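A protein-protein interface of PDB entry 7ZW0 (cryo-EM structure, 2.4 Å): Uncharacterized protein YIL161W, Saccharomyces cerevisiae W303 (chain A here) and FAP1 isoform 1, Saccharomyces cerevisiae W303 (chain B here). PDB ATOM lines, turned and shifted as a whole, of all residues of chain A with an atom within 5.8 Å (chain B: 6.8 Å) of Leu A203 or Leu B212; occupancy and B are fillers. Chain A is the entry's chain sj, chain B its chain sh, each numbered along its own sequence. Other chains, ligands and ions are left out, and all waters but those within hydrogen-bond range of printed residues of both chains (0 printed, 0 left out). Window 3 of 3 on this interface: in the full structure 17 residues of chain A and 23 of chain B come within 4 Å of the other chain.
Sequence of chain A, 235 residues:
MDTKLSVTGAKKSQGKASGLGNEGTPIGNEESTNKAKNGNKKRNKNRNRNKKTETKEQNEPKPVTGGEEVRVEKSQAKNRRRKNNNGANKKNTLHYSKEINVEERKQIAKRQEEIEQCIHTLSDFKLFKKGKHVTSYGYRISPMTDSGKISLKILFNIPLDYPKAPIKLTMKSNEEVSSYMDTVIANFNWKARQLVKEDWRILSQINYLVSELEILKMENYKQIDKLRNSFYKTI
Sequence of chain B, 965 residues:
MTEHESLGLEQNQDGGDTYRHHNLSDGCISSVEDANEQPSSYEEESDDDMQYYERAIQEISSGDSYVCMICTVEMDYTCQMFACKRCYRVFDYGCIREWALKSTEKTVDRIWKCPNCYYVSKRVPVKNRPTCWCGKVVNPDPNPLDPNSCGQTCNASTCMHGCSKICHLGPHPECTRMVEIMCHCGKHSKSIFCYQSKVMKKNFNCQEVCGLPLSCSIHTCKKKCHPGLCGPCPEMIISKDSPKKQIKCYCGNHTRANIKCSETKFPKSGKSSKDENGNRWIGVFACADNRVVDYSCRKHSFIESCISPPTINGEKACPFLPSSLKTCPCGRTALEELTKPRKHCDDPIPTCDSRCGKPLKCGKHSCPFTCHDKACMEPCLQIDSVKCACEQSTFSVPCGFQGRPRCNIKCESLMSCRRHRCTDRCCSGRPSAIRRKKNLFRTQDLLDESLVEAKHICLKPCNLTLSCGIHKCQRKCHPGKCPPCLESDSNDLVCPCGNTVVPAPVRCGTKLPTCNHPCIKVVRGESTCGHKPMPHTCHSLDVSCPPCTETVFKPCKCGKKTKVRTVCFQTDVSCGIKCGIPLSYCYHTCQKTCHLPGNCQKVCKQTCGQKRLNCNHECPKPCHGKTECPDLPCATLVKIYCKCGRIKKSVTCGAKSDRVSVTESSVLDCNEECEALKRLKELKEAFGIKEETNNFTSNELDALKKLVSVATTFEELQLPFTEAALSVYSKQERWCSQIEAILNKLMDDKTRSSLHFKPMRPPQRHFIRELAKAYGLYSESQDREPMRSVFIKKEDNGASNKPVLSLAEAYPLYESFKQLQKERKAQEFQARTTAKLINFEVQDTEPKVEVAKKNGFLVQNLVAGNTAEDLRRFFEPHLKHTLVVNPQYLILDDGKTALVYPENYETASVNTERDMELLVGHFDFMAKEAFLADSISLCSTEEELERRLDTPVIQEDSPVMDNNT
O of Cys B185 lies close to OE1 of Gln A117 (2.7 Å).
The side-chain sulfur (SG) of Cys B230 sits at hydrogen-bond distance from the side-chain sulfur (SG) of Cys B210, 3.7 Å away.
O of Gln A117 sits at hydrogen-bond distance from OG1 of Thr A121 (2.5 Å).
The backbone carbonyl oxygen (O) of Leu B212 is in hydrogen-bond range of the backbone NH (N) of Cys B221.
NZ of Lys B223 is in hydrogen-bond range of O of Cys B230.
Among the printed residues, pairs that only touch across the chains: Leu A203 with Leu B212 (3.7 Å), Leu A203 with Leu B229 (3.9 Å), Ser A204 with Leu B212 (3.999 Å), Ser A204 with Pro B213 (3.5 Å), Ile A206 with Leu B229 (3.5 Å), Asn A207 with Pro B213 (3.9 Å), Asn A207 with Ser B215 (3.98 Å), Asn A207 with Leu B229 (3.9 Å), Asn A207 with Cys B230 (3.7 Å) and Tyr A208 with Ser B215 (3.9 Å).
Of the printed residues of chain A, Leu B212 touches Leu A203 (3.7 Å) and Ser A204 (3.999 Å).
Printed residues of chain B within 4 Å of Gln A117: Cys B185.
Of the printed residues of chain A, Leu B229 touches Leu A203 (3.9 Å), Ile A206 (3.5 Å) and Asn A207 (3.9 Å).
Of the printed residues of chain B, Ile A206 touches Leu B229.
Of the printed residues of chain A, Pro B213 touches Ser A204 (3.5 Å) and Asn A207 (3.9 Å).
The nearest printed residue of chain A that does not touch Cys B230 is Leu A203 (5.5 Å).
Of the 16 printed residues of chain B, 6 touch a printed residue of chain A.
Hydrophobic or aromatic side chains of chain B that line the printed part of chain A: Leu B212, Pro B213 and Leu B229.
Hydrophobic or aromatic side chains of chain A that line the printed part of chain B: Leu A203, Ile A206 and Tyr A208.
Among the printed residues, no Asp or Glu carboxylate lies within 4 Å of a Lys or Arg side-chain nitrogen of the other chain.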
ATOM      1  N   GLN A 117       3.002 -13.649 -19.019  1.00  0.00           N
ATOM      2  CA  GLN A 117       4.392 -13.270 -18.813  1.00  0.00           C
ATOM      3  C   GLN A 117       5.183 -14.399 -18.171  1.00  0.00           C
ATOM      4  O   GLN A 117       6.378 -14.552 -18.440  1.00  0.00           O
ATOM      5  CB  GLN A 117       4.477 -11.991 -17.985  1.00  0.00           C
ATOM      6  CG  GLN A 117       5.852 -11.340 -17.995  1.00  0.00           C
ATOM      7  CD  GLN A 117       6.549 -11.445 -19.339  1.00  0.00           C
ATOM      8  OE1 GLN A 117       7.634 -12.017 -19.441  1.00  0.00           O
ATOM      9  NE2 GLN A 117       5.951 -10.850 -20.371  1.00  0.00           N
ATOM     10  N   CYS A 118       4.534 -15.223 -17.343  1.00  0.00           N
ATOM     11  CA  CYS A 118       5.202 -16.422 -16.846  1.00  0.00           C
ATOM     12  C   CYS A 118       5.453 -17.419 -17.973  1.00  0.00           C
ATOM     13  O   CYS A 118       6.502 -18.078 -18.011  1.00  0.00           O
ATOM     14  CB  CYS A 118       4.377 -17.053 -15.727  1.00  0.00           C
ATOM     15  SG  CYS A 118       4.452 -16.122 -14.186  1.00  0.00           S
ATOM     16  N   THR A 121       8.404 -16.014 -19.824  1.00  0.00           N
ATOM     17  CA  THR A 121       9.653 -16.067 -19.075  1.00  0.00           C
ATOM     18  C   THR A 121      10.204 -17.483 -18.960  1.00  0.00           C
ATOM     19  O   THR A 121      11.414 -17.683 -19.128  1.00  0.00           O
ATOM     20  CB  THR A 121       9.449 -15.468 -17.683  1.00  0.00           C
ATOM     21  OG1 THR A 121       8.748 -14.223 -17.798  1.00  0.00           O
ATOM     22  CG2 THR A 121      10.790 -15.219 -17.007  1.00  0.00           C
ATOM     23  N   LEU A 122       9.356 -18.474 -18.689  1.00  0.00           N
ATOM     24  CA  LEU A 122       9.812 -19.852 -18.505  1.00  0.00           C
ATOM     25  C   LEU A 122       9.338 -20.693 -19.685  1.00  0.00           C
ATOM     26  O   LEU A 122       8.141 -20.739 -19.986  1.00  0.00           O
ATOM     27  CB  LEU A 122       9.331 -20.433 -17.175  1.00  0.00           C
ATOM     28  CG  LEU A 122      10.125 -20.134 -15.893  1.00  0.00           C
ATOM     29  CD1 LEU A 122      11.525 -20.737 -15.988  1.00  0.00           C
ATOM     30  CD2 LEU A 122      10.190 -18.655 -15.517  1.00  0.00           C
ATOM     31  N   ARG A 201       3.995 -11.711  -6.902  1.00  0.00           N
ATOM     32  CA  ARG A 201       3.562 -12.161  -8.215  1.00  0.00           C
ATOM     33  C   ARG A 201       4.075 -13.581  -8.453  1.00  0.00           C
ATOM     34  O   ARG A 201       4.919 -14.077  -7.706  1.00  0.00           O
ATOM     35  CB  ARG A 201       4.066 -11.180  -9.275  1.00  0.00           C
ATOM     36  CG  ARG A 201       3.326 -11.229 -10.585  1.00  0.00           C
ATOM     37  CD  ARG A 201       3.814 -10.181 -11.548  1.00  0.00           C
ATOM     38  NE  ARG A 201       3.565 -10.629 -12.909  1.00  0.00           N
ATOM     39  CZ  ARG A 201       4.367 -11.451 -13.567  1.00  0.00           C
ATOM     40  NH1 ARG A 201       5.493 -11.890 -13.032  1.00  0.00           N
ATOM     41  NH2 ARG A 201       4.025 -11.853 -14.783  1.00  0.00           N
ATOM     42  N   ILE A 202       3.549 -14.242  -9.497  1.00  0.00           N
ATOM     43  CA  ILE A 202       3.763 -15.681  -9.687  1.00  0.00           C
ATOM     44  C   ILE A 202       5.244 -16.003  -9.856  1.00  0.00           C
ATOM     45  O   ILE A 202       5.748 -17.000  -9.312  1.00  0.00           O
ATOM     46  CB  ILE A 202       2.925 -16.191 -10.876  1.00  0.00           C
ATOM     47  CG1 ILE A 202       1.439 -15.973 -10.601  1.00  0.00           C
ATOM     48  CG2 ILE A 202       3.176 -17.674 -11.121  1.00  0.00           C
ATOM     49  CD1 ILE A 202       0.549 -16.197 -11.803  1.00  0.00           C
ATOM     50  N   LEU A 203       5.975 -15.140 -10.567  1.00  0.00           N
ATOM     51  CA  LEU A 203       7.423 -15.305 -10.637  1.00  0.00           C
ATOM     52  C   LEU A 203       8.066 -15.127  -9.265  1.00  0.00           C
ATOM     53  O   LEU A 203       9.060 -15.794  -8.948  1.00  0.00           O
ATOM     54  CB  LEU A 203       8.032 -14.341 -11.656  1.00  0.00           C
ATOM     55  CG  LEU A 203       7.680 -14.536 -13.132  1.00  0.00           C
ATOM     56  CD1 LEU A 203       8.267 -13.413 -13.972  1.00  0.00           C
ATOM     57  CD2 LEU A 203       8.160 -15.881 -13.640  1.00  0.00           C
ATOM     58  N   SER A 204       7.489 -14.270  -8.415  1.00  0.00           N
ATOM     59  CA  SER A 204       8.035 -14.121  -7.069  1.00  0.00           C
ATOM     60  C   SER A 204       7.776 -15.355  -6.207  1.00  0.00           C
ATOM     61  O   SER A 204       8.666 -15.754  -5.449  1.00  0.00           O
ATOM     62  CB  SER A 204       7.487 -12.864  -6.391  1.00  0.00           C
ATOM     63  OG  SER A 204       7.751 -11.709  -7.166  1.00  0.00           O
ATOM     64  N   GLN A 205       6.596 -15.990  -6.311  1.00  0.00           N
ATOM     65  CA  GLN A 205       6.417 -17.242  -5.570  1.00  0.00           C
ATOM     66  C   GLN A 205       7.309 -18.359  -6.098  1.00  0.00           C
ATOM     67  O   GLN A 205       7.795 -19.175  -5.308  1.00  0.00           O
ATOM     68  CB  GLN A 205       4.968 -17.759  -5.525  1.00  0.00           C
ATOM     69  CG  GLN A 205       3.942 -17.020  -4.654  1.00  0.00           C
ATOM     70  CD  GLN A 205       3.218 -15.895  -5.332  1.00  0.00           C
ATOM     71  OE1 GLN A 205       3.179 -15.823  -6.546  1.00  0.00           O
ATOM     72  NE2 GLN A 205       2.587 -15.037  -4.545  1.00  0.00           N
ATOM     73  N   ILE A 206       7.523 -18.453  -7.415  1.00  0.00           N
ATOM     74  CA  ILE A 206       8.346 -19.571  -7.883  1.00  0.00           C
ATOM     75  C   ILE A 206       9.813 -19.337  -7.528  1.00  0.00           C
ATOM     76  O   ILE A 206      10.547 -20.286  -7.218  1.00  0.00           O
ATOM     77  CB  ILE A 206       8.152 -19.851  -9.387  1.00  0.00           C
ATOM     78  CG1 ILE A 206       8.576 -18.678 -10.256  1.00  0.00           C
ATOM     79  CG2 ILE A 206       6.703 -20.200  -9.676  1.00  0.00           C
ATOM     80  CD1 ILE A 206       8.620 -19.002 -11.725  1.00  0.00           C
ATOM     81  N   ASN A 207      10.254 -18.071  -7.524  1.00  0.00           N
ATOM     82  CA  ASN A 207      11.592 -17.757  -7.032  1.00  0.00           C
ATOM     83  C   ASN A 207      11.708 -18.037  -5.539  1.00  0.00           C
ATOM     84  O   ASN A 207      12.738 -18.532  -5.070  1.00  0.00           O
ATOM     85  CB  ASN A 207      11.930 -16.297  -7.334  1.00  0.00           C
ATOM     86  CG  ASN A 207      13.334 -15.927  -6.909  1.00  0.00           C
ATOM     87  OD1 ASN A 207      14.312 -16.414  -7.477  1.00  0.00           O
ATOM     88  ND2 ASN A 207      13.443 -15.066  -5.905  1.00  0.00           N
ATOM     89  N   TYR A 208      10.646 -17.739  -4.789  1.00  0.00           N
ATOM     90  CA  TYR A 208      10.581 -17.998  -3.354  1.00  0.00           C
ATOM     91  C   TYR A 208      10.727 -19.497  -3.081  1.00  0.00           C
ATOM     92  O   TYR A 208      11.516 -19.929  -2.222  1.00  0.00           O
ATOM     93  CB  TYR A 208       9.227 -17.451  -2.884  1.00  0.00           C
ATOM     94  CG  TYR A 208       8.835 -17.489  -1.428  1.00  0.00           C
ATOM     95  CD1 TYR A 208       9.371 -16.579  -0.527  1.00  0.00           C
ATOM     96  CD2 TYR A 208       7.898 -18.399  -0.963  1.00  0.00           C
ATOM     97  CE1 TYR A 208       8.987 -16.578   0.802  1.00  0.00           C
ATOM     98  CE2 TYR A 208       7.520 -18.419   0.367  1.00  0.00           C
ATOM     99  CZ  TYR A 208       8.072 -17.509   1.244  1.00  0.00           C
ATOM    100  OH  TYR A 208       7.700 -17.522   2.568  1.00  0.00           O
ATOM    101  N   CYS B 185      12.820 -10.496 -20.012  1.00  0.00           N
ATOM    102  CA  CYS B 185      11.780 -10.344 -18.990  1.00  0.00           C
ATOM    103  C   CYS B 185      10.370 -10.103 -19.557  1.00  0.00           C
ATOM    104  O   CYS B 185       9.416 -10.050 -18.785  1.00  0.00           O
ATOM    105  CB  CYS B 185      12.196  -9.243 -18.005  1.00  0.00           C
ATOM    106  SG  CYS B 185      12.223  -7.617 -18.817  1.00  0.00           S
ATOM    107  N   VAL B 209      16.002  -3.481 -14.785  1.00  0.00           N
ATOM    108  CA  VAL B 209      16.276  -4.370 -13.657  1.00  0.00           C
ATOM    109  C   VAL B 209      15.081  -5.256 -13.357  1.00  0.00           C
ATOM    110  O   VAL B 209      13.942  -4.793 -13.408  1.00  0.00           O
ATOM    111  CB  VAL B 209      16.582  -3.527 -12.406  1.00  0.00           C
ATOM    112  CG1 VAL B 209      16.976  -4.386 -11.215  1.00  0.00           C
ATOM    113  CG2 VAL B 209      17.659  -2.498 -12.710  1.00  0.00           C
ATOM    114  N   CYS B 210      15.330  -6.526 -13.040  1.00  0.00           N
ATOM    115  CA  CYS B 210      14.241  -7.437 -12.752  1.00  0.00           C
ATOM    116  C   CYS B 210      13.485  -6.908 -11.558  1.00  0.00           C
ATOM    117  O   CYS B 210      12.259  -6.829 -11.594  1.00  0.00           O
ATOM    118  CB  CYS B 210      14.818  -8.800 -12.403  1.00  0.00           C
ATOM    119  SG  CYS B 210      13.594 -10.068 -12.042  1.00  0.00           S
ATOM    120  N   GLY B 211      14.187  -6.546 -10.491  1.00  0.00           N
ATOM    121  CA  GLY B 211      13.543  -5.904  -9.351  1.00  0.00           C
ATOM    122  C   GLY B 211      12.576  -6.751  -8.556  1.00  0.00           C
ATOM    123  O   GLY B 211      11.914  -6.244  -7.652  1.00  0.00           O
ATOM    124  N   LEU B 212      12.496  -8.041  -8.856  1.00  0.00           N
ATOM    125  CA  LEU B 212      11.498  -8.870  -8.191  1.00  0.00           C
ATOM    126  C   LEU B 212      11.899  -9.148  -6.771  1.00  0.00           C
ATOM    127  O   LEU B 212      13.068  -9.360  -6.495  1.00  0.00           O
ATOM    128  CB  LEU B 212      11.253 -10.163  -8.962  1.00  0.00           C
ATOM    129  CG  LEU B 212      10.420 -10.043 -10.241  1.00  0.00           C
ATOM    130  CD1 LEU B 212      10.085 -11.421 -10.791  1.00  0.00           C
ATOM    131  CD2 LEU B 212       9.147  -9.248  -9.992  1.00  0.00           C
ATOM    132  N   PRO B 213      10.923  -9.198  -5.863  1.00  0.00           N
ATOM    133  CA  PRO B 213      11.386  -9.380  -4.490  1.00  0.00           C
ATOM    134  C   PRO B 213      12.167 -10.655  -4.327  1.00  0.00           C
ATOM    135  O   PRO B 213      11.736 -11.720  -4.767  1.00  0.00           O
ATOM    136  CB  PRO B 213      10.087  -9.465  -3.680  1.00  0.00           C
ATOM    137  CG  PRO B 213       8.974  -9.543  -4.678  1.00  0.00           C
ATOM    138  CD  PRO B 213       9.485  -8.912  -5.933  1.00  0.00           C
ATOM    139  N   LEU B 214      13.314 -10.551  -3.676  1.00  0.00           N
ATOM    140  CA  LEU B 214      14.124 -11.724  -3.420  1.00  0.00           C
ATOM    141  C   LEU B 214      13.455 -12.514  -2.323  1.00  0.00           C
ATOM    142  O   LEU B 214      12.627 -11.978  -1.598  1.00  0.00           O
ATOM    143  CB  LEU B 214      15.555 -11.338  -3.070  1.00  0.00           C
ATOM    144  CG  LEU B 214      16.360 -10.948  -4.312  1.00  0.00           C
ATOM    145  CD1 LEU B 214      17.670 -10.243  -4.006  1.00  0.00           C
ATOM    146  CD2 LEU B 214      16.582 -12.137  -5.231  1.00  0.00           C
ATOM    147  N   SER B 215      13.823 -13.772  -2.164  1.00  0.00           N
ATOM    148  CA  SER B 215      13.131 -14.639  -1.211  1.00  0.00           C
ATOM    149  C   SER B 215      13.155 -14.148   0.223  1.00  0.00           C
ATOM    150  O   SER B 215      12.184 -14.331   0.954  1.00  0.00           O
ATOM    151  CB  SER B 215      13.720 -16.034  -1.291  1.00  0.00           C
ATOM    152  OG  SER B 215      15.137 -15.967  -1.255  1.00  0.00           O
ATOM    153  N   HIS B 219      14.840  -7.870   0.203  1.00  0.00           N
ATOM    154  CA  HIS B 219      15.626  -7.497  -0.959  1.00  0.00           C
ATOM    155  C   HIS B 219      14.838  -7.675  -2.239  1.00  0.00           C
ATOM    156  O   HIS B 219      13.830  -8.377  -2.252  1.00  0.00           O
ATOM    157  CB  HIS B 219      16.904  -8.324  -1.027  1.00  0.00           C
ATOM    158  CG  HIS B 219      17.959  -7.900  -0.058  1.00  0.00           C
ATOM    159  ND1 HIS B 219      18.197  -8.567   1.125  1.00  0.00           N
ATOM    160  CD2 HIS B 219      18.851  -6.880  -0.100  1.00  0.00           C
ATOM    161  CE1 HIS B 219      19.190  -7.978   1.768  1.00  0.00           C
ATOM    162  NE2 HIS B 219      19.602  -6.949   1.049  1.00  0.00           N
ATOM    163  N   THR B 220      15.261  -7.003  -3.301  1.00  0.00           N
ATOM    164  CA  THR B 220      14.620  -7.174  -4.595  1.00  0.00           C
ATOM    165  C   THR B 220      15.742  -7.541  -5.528  1.00  0.00           C
ATOM    166  O   THR B 220      16.871  -7.082  -5.344  1.00  0.00           O
ATOM    167  CB  THR B 220      13.953  -5.889  -5.109  1.00  0.00           C
ATOM    168  OG1 THR B 220      14.961  -4.947  -5.495  1.00  0.00           O
ATOM    169  CG2 THR B 220      13.072  -5.272  -4.034  1.00  0.00           C
ATOM    170  N   CYS B 221      15.455  -8.356  -6.533  1.00  0.00           N
ATOM    171  CA  CYS B 221      16.519  -8.815  -7.391  1.00  0.00           C
ATOM    172  C   CYS B 221      17.152  -7.604  -8.011  1.00  0.00           C
ATOM    173  O   CYS B 221      16.472  -6.726  -8.528  1.00  0.00           O
ATOM    174  CB  CYS B 221      15.956  -9.722  -8.465  1.00  0.00           C
ATOM    175  SG  CYS B 221      17.169 -10.229  -9.695  1.00  0.00           S
ATOM    176  N   LYS B 222      18.470  -7.550  -7.952  1.00  0.00           N
ATOM    177  CA  LYS B 222      19.161  -6.405  -8.489  1.00  0.00           C
ATOM    178  C   LYS B 222      19.573  -6.679  -9.912  1.00  0.00           C
ATOM    179  O   LYS B 222      20.115  -5.808 -10.584  1.00  0.00           O
ATOM    180  CB  LYS B 222      20.351  -6.045  -7.605  1.00  0.00           C
ATOM    181  CG  LYS B 222      19.906  -5.467  -6.276  1.00  0.00           C
ATOM    182  CD  LYS B 222      20.984  -4.633  -5.609  1.00  0.00           C
ATOM    183  CE  LYS B 222      20.439  -3.969  -4.354  1.00  0.00           C
ATOM    184  NZ  LYS B 222      21.429  -3.059  -3.714  1.00  0.00           N
ATOM    185  N   LYS B 223      19.307  -7.891 -10.380  1.00  0.00           N
ATOM    186  CA  LYS B 223      19.714  -8.251 -11.726  1.00  0.00           C
ATOM    187  C   LYS B 223      18.901  -7.506 -12.768  1.00  0.00           C
ATOM    188  O   LYS B 223      17.756  -7.174 -12.518  1.00  0.00           O
ATOM    189  CB  LYS B 223      19.617  -9.757 -11.958  1.00  0.00           C
ATOM    190  CG  LYS B 223      20.644 -10.580 -11.208  1.00  0.00           C
ATOM    191  CD  LYS B 223      20.449 -12.056 -11.503  1.00  0.00           C
ATOM    192  CE  LYS B 223      21.469 -12.905 -10.768  1.00  0.00           C
ATOM    193  NZ  LYS B 223      21.240 -14.360 -10.986  1.00  0.00           N
ATOM    194  N   GLY B 228      15.056 -16.572 -17.250  1.00  0.00           N
ATOM    195  CA  GLY B 228      15.030 -17.376 -16.044  1.00  0.00           C
ATOM    196  C   GLY B 228      14.748 -16.614 -14.762  1.00  0.00           C
ATOM    197  O   GLY B 228      14.452 -15.424 -14.803  1.00  0.00           O
ATOM    198  N   LEU B 229      14.834 -17.289 -13.618  1.00  0.00           N
ATOM    199  CA  LEU B 229      14.527 -16.666 -12.318  1.00  0.00           C
ATOM    200  C   LEU B 229      15.562 -15.718 -11.738  1.00  0.00           C
ATOM    201  O   LEU B 229      16.730 -15.763 -12.118  1.00  0.00           O
ATOM    202  CB  LEU B 229      14.243 -17.746 -11.283  1.00  0.00           C
ATOM    203  CG  LEU B 229      12.918 -18.478 -11.444  1.00  0.00           C
ATOM    204  CD1 LEU B 229      12.904 -19.736 -10.595  1.00  0.00           C
ATOM    205  CD2 LEU B 229      11.792 -17.546 -11.050  1.00  0.00           C
ATOM    206  N   CYS B 230      15.147 -14.889 -10.782  1.00  0.00           N
ATOM    207  CA  CYS B 230      16.060 -13.943 -10.143  1.00  0.00           C
ATOM    208  C   CYS B 230      17.175 -14.697  -9.462  1.00  0.00           C
ATOM    209  O   CYS B 230      18.321 -14.252  -9.462  1.00  0.00           O
ATOM    210  CB  CYS B 230      15.316 -13.148  -9.083  1.00  0.00           C
ATOM    211  SG  CYS B 230      13.604 -12.772  -9.497  1.00  0.00           S
